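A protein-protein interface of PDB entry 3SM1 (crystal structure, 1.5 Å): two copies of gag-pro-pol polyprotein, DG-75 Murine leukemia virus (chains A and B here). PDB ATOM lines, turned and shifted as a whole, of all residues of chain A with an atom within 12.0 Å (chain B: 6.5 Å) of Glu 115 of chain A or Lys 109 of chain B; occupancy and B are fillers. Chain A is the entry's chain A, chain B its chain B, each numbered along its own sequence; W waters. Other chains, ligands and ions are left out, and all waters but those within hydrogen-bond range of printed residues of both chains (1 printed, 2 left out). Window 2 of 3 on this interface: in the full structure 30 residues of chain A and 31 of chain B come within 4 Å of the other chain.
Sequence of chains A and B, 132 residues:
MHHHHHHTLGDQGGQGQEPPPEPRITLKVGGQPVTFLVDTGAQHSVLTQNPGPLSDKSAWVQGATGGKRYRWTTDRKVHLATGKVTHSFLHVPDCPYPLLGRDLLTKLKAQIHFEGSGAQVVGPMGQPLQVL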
ATOM      1  N   PRO A  21      23.821  20.352  11.822  1.00  0.00           N
ATOM      2  CA  PRO A  21      23.505  21.046  13.057  1.00  0.00           C
ATOM      3  C   PRO A  21      23.311  20.076  14.227  1.00  0.00           C
ATOM      4  O   PRO A  21      23.149  18.854  14.010  1.00  0.00           O
ATOM      5  CB  PRO A  21      22.161  21.715  12.746  1.00  0.00           C
ATOM      6  CG  PRO A  21      21.593  20.929  11.690  1.00  0.00           C
ATOM      7  CD  PRO A  21      22.712  20.398  10.851  1.00  0.00           C
ATOM      8  N   GLU A  22      23.339  20.601  15.443  1.00  0.00           N
ATOM      9  CA  GLU A  22      23.001  19.813  16.613  1.00  0.00           C
ATOM     10  C   GLU A  22      21.489  19.527  16.560  1.00  0.00           C
ATOM     11  O   GLU A  22      20.718  20.394  16.127  1.00  0.00           O
ATOM     12  CB  GLU A  22      23.345  20.574  17.891  1.00  0.00           C
ATOM     13  CG  GLU A  22      24.850  20.872  18.072  1.00  0.00           C
ATOM     14  CD  GLU A  22      25.134  21.510  19.423  1.00  0.00           C
ATOM     15  OE1 GLU A  22      24.227  22.141  19.972  1.00  0.00           O
ATOM     16  OE2 GLU A  22      26.258  21.365  19.949  1.00  0.00           O
ATOM     17  N   PRO A  23      21.052  18.359  17.043  1.00  0.00           N
ATOM     18  CA  PRO A  23      21.849  17.302  17.671  1.00  0.00           C
ATOM     19  C   PRO A  23      22.547  16.429  16.651  1.00  0.00           C
ATOM     20  O   PRO A  23      21.960  16.083  15.619  1.00  0.00           O
ATOM     21  CB  PRO A  23      20.802  16.505  18.472  1.00  0.00           C
ATOM     22  CG  PRO A  23      19.507  16.680  17.691  1.00  0.00           C
ATOM     23  CD  PRO A  23      19.598  18.077  17.086  1.00  0.00           C
ATOM     24  N   ARG A  24      23.814  16.159  16.899  1.00  0.00           N
ATOM     25  CA  ARG A  24      24.605  15.384  15.988  1.00  0.00           C
ATOM     26  C   ARG A  24      25.465  14.409  16.781  1.00  0.00           C
ATOM     27  O   ARG A  24      25.721  14.615  17.961  1.00  0.00           O
ATOM     28  CB  ARG A  24      25.481  16.282  15.092  1.00  0.00           C
ATOM     29  CG  ARG A  24      26.516  17.071  15.856  1.00  0.00           C
ATOM     30  CD  ARG A  24      27.479  17.799  14.908  1.00  0.00           C
ATOM     31  NE  ARG A  24      28.235  18.781  15.677  1.00  0.00           N
ATOM     32  CZ  ARG A  24      28.023  20.096  15.675  1.00  0.00           C
ATOM     33  NH1 ARG A  24      27.116  20.656  14.900  1.00  0.00           N
ATOM     34  NH2 ARG A  24      28.774  20.872  16.443  1.00  0.00           N
ATOM     35  N   GLN A 111      18.957   9.687  24.712  1.00  0.00           N
ATOM     36  CA  GLN A 111      18.167  10.852  25.100  1.00  0.00           C
ATOM     37  C   GLN A 111      18.724  12.049  24.339  1.00  0.00           C
ATOM     38  O   GLN A 111      19.928  12.144  24.103  1.00  0.00           O
ATOM     39  CB  GLN A 111      18.304  11.121  26.593  1.00  0.00           C
ATOM     40  CG  GLN A 111      17.873   9.965  27.452  1.00  0.00           C
ATOM     41  CD  GLN A 111      18.271  10.153  28.899  1.00  0.00           C
ATOM     42  OE1 GLN A 111      18.349  11.278  29.397  1.00  0.00           O
ATOM     43  NE2 GLN A 111      18.526   9.046  29.587  1.00  0.00           N
ATOM     44  N   ILE A 112      17.854  12.972  23.959  1.00  0.00           N
ATOM     45  CA  ILE A 112      18.282  14.169  23.265  1.00  0.00           C
ATOM     46  C   ILE A 112      17.783  15.337  24.086  1.00  0.00           C
ATOM     47  O   ILE A 112      16.571  15.433  24.338  1.00  0.00           O
ATOM     48  CB  ILE A 112      17.689  14.262  21.825  1.00  0.00           C
ATOM     49  CG1 ILE A 112      18.068  12.992  21.037  1.00  0.00           C
ATOM     50  CG2 ILE A 112      18.204  15.518  21.131  1.00  0.00           C
ATOM     51  CD1 ILE A 112      17.112  12.611  19.981  1.00  0.00           C
ATOM     52  N   HIS A 113      18.704  16.181  24.549  1.00  0.00           N
ATOM     53  CA  HIS A 113      18.361  17.278  25.451  1.00  0.00           C
ATOM     54  C   HIS A 113      18.571  18.605  24.778  1.00  0.00           C
ATOM     55  O   HIS A 113      19.683  18.922  24.333  1.00  0.00           O
ATOM     56  CB  HIS A 113      19.282  17.238  26.672  1.00  0.00           C
ATOM     57  CG  HIS A 113      19.062  16.066  27.569  1.00  0.00           C
ATOM     58  ND1 HIS A 113      18.709  16.211  28.892  1.00  0.00           N
ATOM     59  CD2 HIS A 113      19.137  14.734  27.346  1.00  0.00           C
ATOM     60  CE1 HIS A 113      18.586  15.019  29.451  1.00  0.00           C
ATOM     61  NE2 HIS A 113      18.839  14.104  28.536  1.00  0.00           N
ATOM     62  N   PHE A 114      17.518  19.410  24.714  1.00  0.00           N
ATOM     63  CA  PHE A 114      17.623  20.762  24.168  1.00  0.00           C
ATOM     64  C   PHE A 114      18.000  21.747  25.277  1.00  0.00           C
ATOM     65  O   PHE A 114      17.296  21.855  26.261  1.00  0.00           O
ATOM     66  CB  PHE A 114      16.348  21.124  23.386  1.00  0.00           C
ATOM     67  CG  PHE A 114      16.320  20.497  22.029  1.00  0.00           C
ATOM     68  CD1 PHE A 114      16.674  21.238  20.916  1.00  0.00           C
ATOM     69  CD2 PHE A 114      15.977  19.147  21.869  1.00  0.00           C
ATOM     70  CE1 PHE A 114      16.663  20.664  19.629  1.00  0.00           C
ATOM     71  CE2 PHE A 114      16.000  18.547  20.582  1.00  0.00           C
ATOM     72  CZ  PHE A 114      16.338  19.313  19.475  1.00  0.00           C
ATOM     73  N   GLU A 115      19.177  22.356  25.151  1.00  0.00           N
ATOM     74  CA  GLU A 115      19.694  23.281  26.183  1.00  0.00           C
ATOM     75  C   GLU A 115      20.517  24.381  25.547  1.00  0.00           C
ATOM     76  O   GLU A 115      21.346  24.115  24.677  1.00  0.00           O
ATOM     77  CB  GLU A 115      20.541  22.553  27.239  1.00  0.00           C
ATOM     78  CG  GLU A 115      19.760  21.746  28.296  1.00  0.00           C
ATOM     79  CD  GLU A 115      18.583  22.505  28.938  1.00  0.00           C
ATOM     80  OE1 GLU A 115      17.530  21.866  29.181  1.00  0.00           O
ATOM     81  OE2 GLU A 115      18.704  23.726  29.201  1.00  0.00           O
ATOM     82  N   GLY A 116      20.297  25.617  25.992  1.00  0.00           N
ATOM     83  CA  GLY A 116      20.824  26.779  25.279  1.00  0.00           C
ATOM     84  C   GLY A 116      20.173  26.861  23.911  1.00  0.00           C
ATOM     85  O   GLY A 116      18.964  26.639  23.776  1.00  0.00           O
ATOM     86  N   SER A 117      20.978  27.170  22.898  1.00  0.00           N
ATOM     87  CA  SER A 117      20.507  27.199  21.510  1.00  0.00           C
ATOM     88  C   SER A 117      20.817  25.864  20.813  1.00  0.00           C
ATOM     89  O   SER A 117      20.520  25.677  19.623  1.00  0.00           O
ATOM     90  CB  SER A 117      21.151  28.366  20.745  1.00  0.00           C
ATOM     91  OG  SER A 117      22.567  28.226  20.670  1.00  0.00           O
ATOM     92  N   GLY A 118      21.403  24.939  21.573  1.00  0.00           N
ATOM     93  CA  GLY A 118      21.854  23.669  21.024  1.00  0.00           C
ATOM     94  C   GLY A 118      21.147  22.445  21.575  1.00  0.00           C
ATOM     95  O   GLY A 118      20.062  22.527  22.186  1.00  0.00           O
ATOM     96  N   ALA A 119      21.768  21.294  21.338  1.00  0.00           N
ATOM     97  CA  ALA A 119      21.168  20.025  21.712  1.00  0.00           C
ATOM     98  C   ALA A 119      22.284  19.032  21.903  1.00  0.00           C
ATOM     99  O   ALA A 119      23.259  19.035  21.155  1.00  0.00           O
ATOM    100  CB  ALA A 119      20.230  19.542  20.622  1.00  0.00           C
ATOM    101  N   GLN A 120      22.122  18.204  22.921  1.00  0.00           N
ATOM    102  CA  GLN A 120      23.130  17.238  23.297  1.00  0.00           C
ATOM    103  C   GLN A 120      22.502  15.867  23.353  1.00  0.00           C
ATOM    104  O   GLN A 120      21.397  15.690  23.850  1.00  0.00           O
ATOM    105  CB  GLN A 120      23.730  17.611  24.652  1.00  0.00           C
ATOM    106  CG  GLN A 120      24.788  16.625  25.150  1.00  0.00           C
ATOM    107  CD  GLN A 120      26.098  17.294  25.491  1.00  0.00           C
ATOM    108  OE1 GLN A 120      26.594  17.175  26.616  1.00  0.00           O
ATOM    109  NE2 GLN A 120      26.671  18.007  24.519  1.00  0.00           N
ATOM    110  N   VAL A 121      23.224  14.887  22.829  1.00  0.00           N
ATOM    111  CA  VAL A 121      22.787  13.494  22.889  1.00  0.00           C
ATOM    112  C   VAL A 121      23.452  12.842  24.112  1.00  0.00           C
ATOM    113  O   VAL A 121      24.641  13.053  24.371  1.00  0.00           O
ATOM    114  CB  VAL A 121      23.182  12.740  21.621  1.00  0.00           C
ATOM    115  CG1 VAL A 121      22.696  11.292  21.684  1.00  0.00           C
ATOM    116  CG2 VAL A 121      22.658  13.484  20.374  1.00  0.00           C
ATOM    117  N   VAL A 122      22.667  12.059  24.832  1.00  0.00           N
ATOM    118  CA  VAL A 122      23.093  11.392  26.051  1.00  0.00           C
ATOM    119  C   VAL A 122      22.727   9.904  25.924  1.00  0.00           C
ATOM    120  O   VAL A 122      21.675   9.545  25.361  1.00  0.00           O
ATOM    121  CB  VAL A 122      22.385  12.042  27.251  1.00  0.00           C
ATOM    122  CG1 VAL A 122      22.761  11.361  28.522  1.00  0.00           C
ATOM    123  CG2 VAL A 122      22.750  13.518  27.353  1.00  0.00           C
ATOM    124  N   PRO A 128      27.492  11.612  28.082  1.00  0.00           N
ATOM    125  CA  PRO A 128      27.330  12.496  26.926  1.00  0.00           C
ATOM    126  C   PRO A 128      27.939  11.894  25.653  1.00  0.00           C
ATOM    127  O   PRO A 128      29.072  11.391  25.694  1.00  0.00           O
ATOM    128  CB  PRO A 128      28.121  13.750  27.330  1.00  0.00           C
ATOM    129  CG  PRO A 128      28.205  13.696  28.794  1.00  0.00           C
ATOM    130  CD  PRO A 128      28.308  12.250  29.132  1.00  0.00           C
ATOM    131  N   LEU B 104      11.016  24.986  17.936  1.00  0.00           N
ATOM    132  CA  LEU B 104      10.140  24.918  19.108  1.00  0.00           C
ATOM    133  C   LEU B 104      10.703  23.991  20.206  1.00  0.00           C
ATOM    134  O   LEU B 104      10.401  24.163  21.403  1.00  0.00           O
ATOM    135  CB  LEU B 104       8.706  24.546  18.719  1.00  0.00           C
ATOM    136  CG  LEU B 104       7.992  25.685  17.987  1.00  0.00           C
ATOM    137  CD1 LEU B 104       6.657  25.248  17.448  1.00  0.00           C
ATOM    138  CD2 LEU B 104       7.760  26.826  18.969  1.00  0.00           C
ATOM    139  N   LEU B 105      11.517  23.007  19.825  1.00  0.00           N
ATOM    140  CA  LEU B 105      12.157  22.154  20.828  1.00  0.00           C
ATOM    141  C   LEU B 105      13.086  22.981  21.714  1.00  0.00           C
ATOM    142  O   LEU B 105      13.166  22.726  22.935  1.00  0.00           O
ATOM    143  CB  LEU B 105      12.891  20.982  20.196  1.00  0.00           C
ATOM    144  CG  LEU B 105      11.971  19.941  19.556  1.00  0.00           C
ATOM    145  CD1 LEU B 105      12.699  18.977  18.626  1.00  0.00           C
ATOM    146  CD2 LEU B 105      11.222  19.160  20.641  1.00  0.00           C
ATOM    147  N   THR B 106      13.746  23.983  21.137  1.00  0.00           N
ATOM    148  CA  THR B 106      14.584  24.911  21.914  1.00  0.00           C
ATOM    149  C   THR B 106      13.733  25.739  22.865  1.00  0.00           C
ATOM    150  O   THR B 106      14.091  25.891  24.035  1.00  0.00           O
ATOM    151  CB  THR B 106      15.358  25.799  20.981  1.00  0.00           C
ATOM    152  OG1 THR B 106      16.382  25.018  20.364  1.00  0.00           O
ATOM    153  CG2 THR B 106      16.046  26.938  21.755  1.00  0.00           C
ATOM    154  N   LYS B 107      12.603  26.238  22.371  1.00  0.00           N
ATOM    155  CA  LYS B 107      11.713  27.073  23.195  1.00  0.00           C
ATOM    156  C   LYS B 107      11.109  26.279  24.346  1.00  0.00           C
ATOM    157  O   LYS B 107      10.940  26.814  25.456  1.00  0.00           O
ATOM    158  CB  LYS B 107      10.609  27.713  22.350  1.00  0.00           C
ATOM    159  CG  LYS B 107      11.096  28.773  21.390  1.00  0.00           C
ATOM    160  CD  LYS B 107       9.920  29.530  20.775  1.00  0.00           C
ATOM    161  CE  LYS B 107      10.395  30.616  19.823  1.00  0.00           C
ATOM    162  NZ  LYS B 107       9.205  31.295  19.170  1.00  0.00           N
ATOM    163  N   LEU B 108      10.802  25.002  24.102  1.00  0.00           N
ATOM    164  CA  LEU B 108      10.314  24.076  25.133  1.00  0.00           C
ATOM    165  C   LEU B 108      11.413  23.549  26.066  1.00  0.00           C
ATOM    166  O   LEU B 108      11.087  22.971  27.100  1.00  0.00           O
ATOM    167  CB  LEU B 108       9.656  22.854  24.473  1.00  0.00           C
ATOM    168  CG  LEU B 108       8.274  23.007  23.867  1.00  0.00           C
ATOM    169  CD1 LEU B 108       7.974  21.933  22.817  1.00  0.00           C
ATOM    170  CD2 LEU B 108       7.200  23.006  24.969  1.00  0.00           C
ATOM    171  N   LYS B 109      12.683  23.729  25.693  1.00  0.00           N
ATOM    172  CA  LYS B 109      13.822  23.062  26.338  1.00  0.00           C
ATOM    173  C   LYS B 109      13.523  21.575  26.551  1.00  0.00           C
ATOM    174  O   LYS B 109      13.762  21.008  27.624  1.00  0.00           O
ATOM    175  CB  LYS B 109      14.200  23.774  27.659  1.00  0.00           C
ATOM    176  CG  LYS B 109      14.668  25.232  27.494  1.00  0.00           C
ATOM    177  CD  LYS B 109      16.126  25.301  27.020  1.00  0.00           C
ATOM    178  CE  LYS B 109      16.653  26.742  26.999  1.00  0.00           C
ATOM    179  NZ  LYS B 109      16.195  27.488  25.789  1.00  0.00           N
ATOM    180  N   ALA B 110      12.986  20.940  25.505  1.00  0.00           N
ATOM    181  CA  ALA B 110      12.534  19.571  25.559  1.00  0.00           C
ATOM    182  C   ALA B 110      13.669  18.570  25.698  1.00  0.00           C
ATOM    183  O   ALA B 110      14.804  18.830  25.267  1.00  0.00           O
ATOM    184  CB  ALA B 110      11.710  19.247  24.306  1.00  0.00           C
ATOM    185  N   GLN B 111      13.319  17.420  26.273  1.00  0.00           N
ATOM    186  CA  GLN B 111      14.152  16.215  26.216  1.00  0.00           C
ATOM    187  C   GLN B 111      13.360  15.129  25.531  1.00  0.00           C
ATOM    188  O   GLN B 111      12.148  15.018  25.712  1.00  0.00           O
ATOM    189  CB  GLN B 111      14.516  15.703  27.604  1.00  0.00           C
ATOM    190  CG  GLN B 111      15.115  16.735  28.521  1.00  0.00           C
ATOM    191  CD  GLN B 111      15.328  16.157  29.921  1.00  0.00           C
ATOM    192  OE1 GLN B 111      15.332  14.941  30.104  1.00  0.00           O
ATOM    193  NE2 GLN B 111      15.522  17.025  30.904  1.00  0.00           N
ATOM    194  N   VAL B 122       9.645  15.038  27.062  1.00  0.00           N
ATOM    195  CA  VAL B 122       9.445  15.680  28.349  1.00  0.00           C
ATOM    196  C   VAL B 122      10.019  17.100  28.361  1.00  0.00           C
ATOM    197  O   VAL B 122      10.770  17.504  27.440  1.00  0.00           O
ATOM    198  CB  VAL B 122      10.034  14.806  29.475  1.00  0.00           C
ATOM    199  CG1 VAL B 122       9.328  13.443  29.520  1.00  0.00           C
ATOM    200  CG2 VAL B 122      11.515  14.612  29.300  1.00  0.00           C
ATOM    201  N   GLY B 123       9.652  17.880  29.395  1.00  0.00           N
ATOM    202  CA  GLY B 123      10.230  19.207  29.653  1.00  0.00           C
ATOM    203  C   GLY B 123      11.646  19.218  30.221  1.00  0.00           C
ATOM    204  O   GLY B 123      12.257  18.160  30.423  1.00  0.00           O
ATOM    205  N   PRO B 124      12.199  20.427  30.467  1.00  0.00           N
ATOM    206  CA  PRO B 124      13.607  20.610  30.848  1.00  0.00           C
ATOM    207  C   PRO B 124      13.954  19.911  32.161  1.00  0.00           C
ATOM    208  O   PRO B 124      15.115  19.552  32.402  1.00  0.00           O
ATOM    209  CB  PRO B 124      13.758  22.132  30.991  1.00  0.00           C
ATOM    210  CG  PRO B 124      12.371  22.670  31.045  1.00  0.00           C
ATOM    211  CD  PRO B 124      11.461  21.701  30.365  1.00  0.00           C
ATOM    212  N   MET B 125      12.938  19.712  32.991  1.00  0.00           N
ATOM    213  CA  MET B 125      13.100  18.885  34.178  1.00  0.00           C
ATOM    214  C   MET B 125      12.194  17.680  34.206  1.00  0.00           C
ATOM    215  O   MET B 125      11.707  17.295  35.266  1.00  0.00           O
ATOM    216  CB  MET B 125      12.926  19.703  35.431  1.00  0.00           C
ATOM    217  CG  MET B 125      14.192  20.424  35.782  1.00  0.00           C
ATOM    218  SD  MET B 125      13.746  21.818  36.758  1.00  0.00           S
ATOM    219  CE  MET B 125      12.755  22.716  35.545  1.00  0.00           C
HETATM  220  O   HOH W   1      18.190  24.419  22.354  1.00  0.00           O
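N of Phe 114 of chain A sits at hydrogen-bond distance from O of Ala 110 of chain B (2.8 Å).
The side-chain amide oxygen (OE1) of Gln 111 of chain A sits at hydrogen-bond distance from a ring nitrogen (NE2) of His 113 of chain A (3.0 Å). The backbone carbonyl oxygen (O) of Gln 120 of chain A is in hydrogen-bond range of the backbone NH (N) of His 113 of chain A (2.8 Å). The backbone carbonyl oxygen of Thr 106 of chain B sits at hydrogen-bond distance from the side-chain amino group of Lys 109 of chain B (3.2 Å). The backbone NH (N) of Gln 111 of chain B sits at hydrogen-bond distance from the backbone carbonyl oxygen (O) of Val 122 of chain B (2.8 Å). The side-chain amide nitrogen of Gln 111 of chain B is in hydrogen-bond range of the backbone carbonyl oxygen of Gly 123 of chain B, 3.5 Å away. The backbone carbonyl oxygen (O) of Pro 124 of chain B lies within hydrogen-bond range of the side-chain amide nitrogen (NE2) of Gln 111 of chain B, at 3.0 Å.
O of Ile 112 of chain A touches O of Ala 110 of chain B (3.9 Å). Ile 112 of chain A touches Gln 111 of chain B (O to CA, 3.2 Å). O of Ala 110 of chain B touches C of His 113 of chain A (3.8 Å). Gln 111 of chain B touches His 113 of chain A. Leu 105 of chain B touches Phe 114 of chain A (O to CB, 3.6 Å). Thr 106 of chain B touches Phe 114 of chain A. Phe 114 of chain A touches Lys 109 of chain B. Glu 115 of chain A touches Lys 109 of chain B (OE2 to CD, 3.7 Å). O of Gly 116 of chain A touches CG2 of Thr 106 of chain B, at 3.6 Å. Gly 116 of chain A touches Lys 109 of chain B (O to NZ, 3.5 Å).
Of the printed residues of chain B, Ile 112 of chain A touches Ala 110 (3.9 Å) and Gln 111 (3.2 Å). Of the printed residues of chain B, Phe 114 of chain A touches Leu 105 (3.6 Å), Thr 106 (3.8 Å), Lys 109 (3.7 Å) and Ala 110 (2.8 Å). Glu 115 of chain A touches one residue of chain B. Printed residues of chain B within 4 Å of Gly 116 of chain A: Thr 106 (3.6 Å) and Lys 109 (3.5 Å). Of the printed residues of chain A, Leu 105 of chain B touches Phe 114. No residue of chain A comes within 4 Å of Leu 108 of chain B. Of the printed residues of chain A, Lys 109 of chain B touches Phe 114 (3.7 Å), Glu 115 (3.7 Å) and Gly 116 (3.5 Å). Ala 110 of chain B touches just these residues of chain A: Ile 112 (3.9 Å), His 113 (3.8 Å) and Phe 114 (2.8 Å). No residue of chain A comes within 4 Å of Gly 123 of chain B. The nearest residue of chain B that does not touch Glu 115 of chain A is Pro 124 of chain B (4.2 Å). The nearest residue of chain A that does not touch Lys 109 of chain B is Ser 117 of chain A (5.6 Å). The nearest printed residue of chain B that does not touch Gly 116 of chain A is Lys 107 of chain B (6.5 Å).
Printed residues of chain B that touch a printed residue of chain A: Leu 105, Thr 106, Lys 109, Ala 110 and Gln 111. Hydrophobic or aromatic side chains of chain B within 4 Å of the printed part of chain A: Leu 105. Printed residues of chain A that touch a printed residue of chain B: Ile 112, His 113, Phe 114, Glu 115 and Gly 116. Hydrophobic or aromatic side chains of chain A within 4 Å of the printed part of chain B: His 113 and Phe 114. Among the printed residues, 11 pairs touch across the chains. Among the printed residues, no Asp or Glu carboxylate lies within 4 Å of a Lys or Arg side-chain nitrogen of the other chain.
2 positions are printed for both chains.
Water W1 lies within hydrogen-bond range of O of Gly 118 of chain A (2.7 Å), O of Gly 116 of chain A (2.7 Å) and OG1 of Thr 106 of chain B (2.8 Å).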
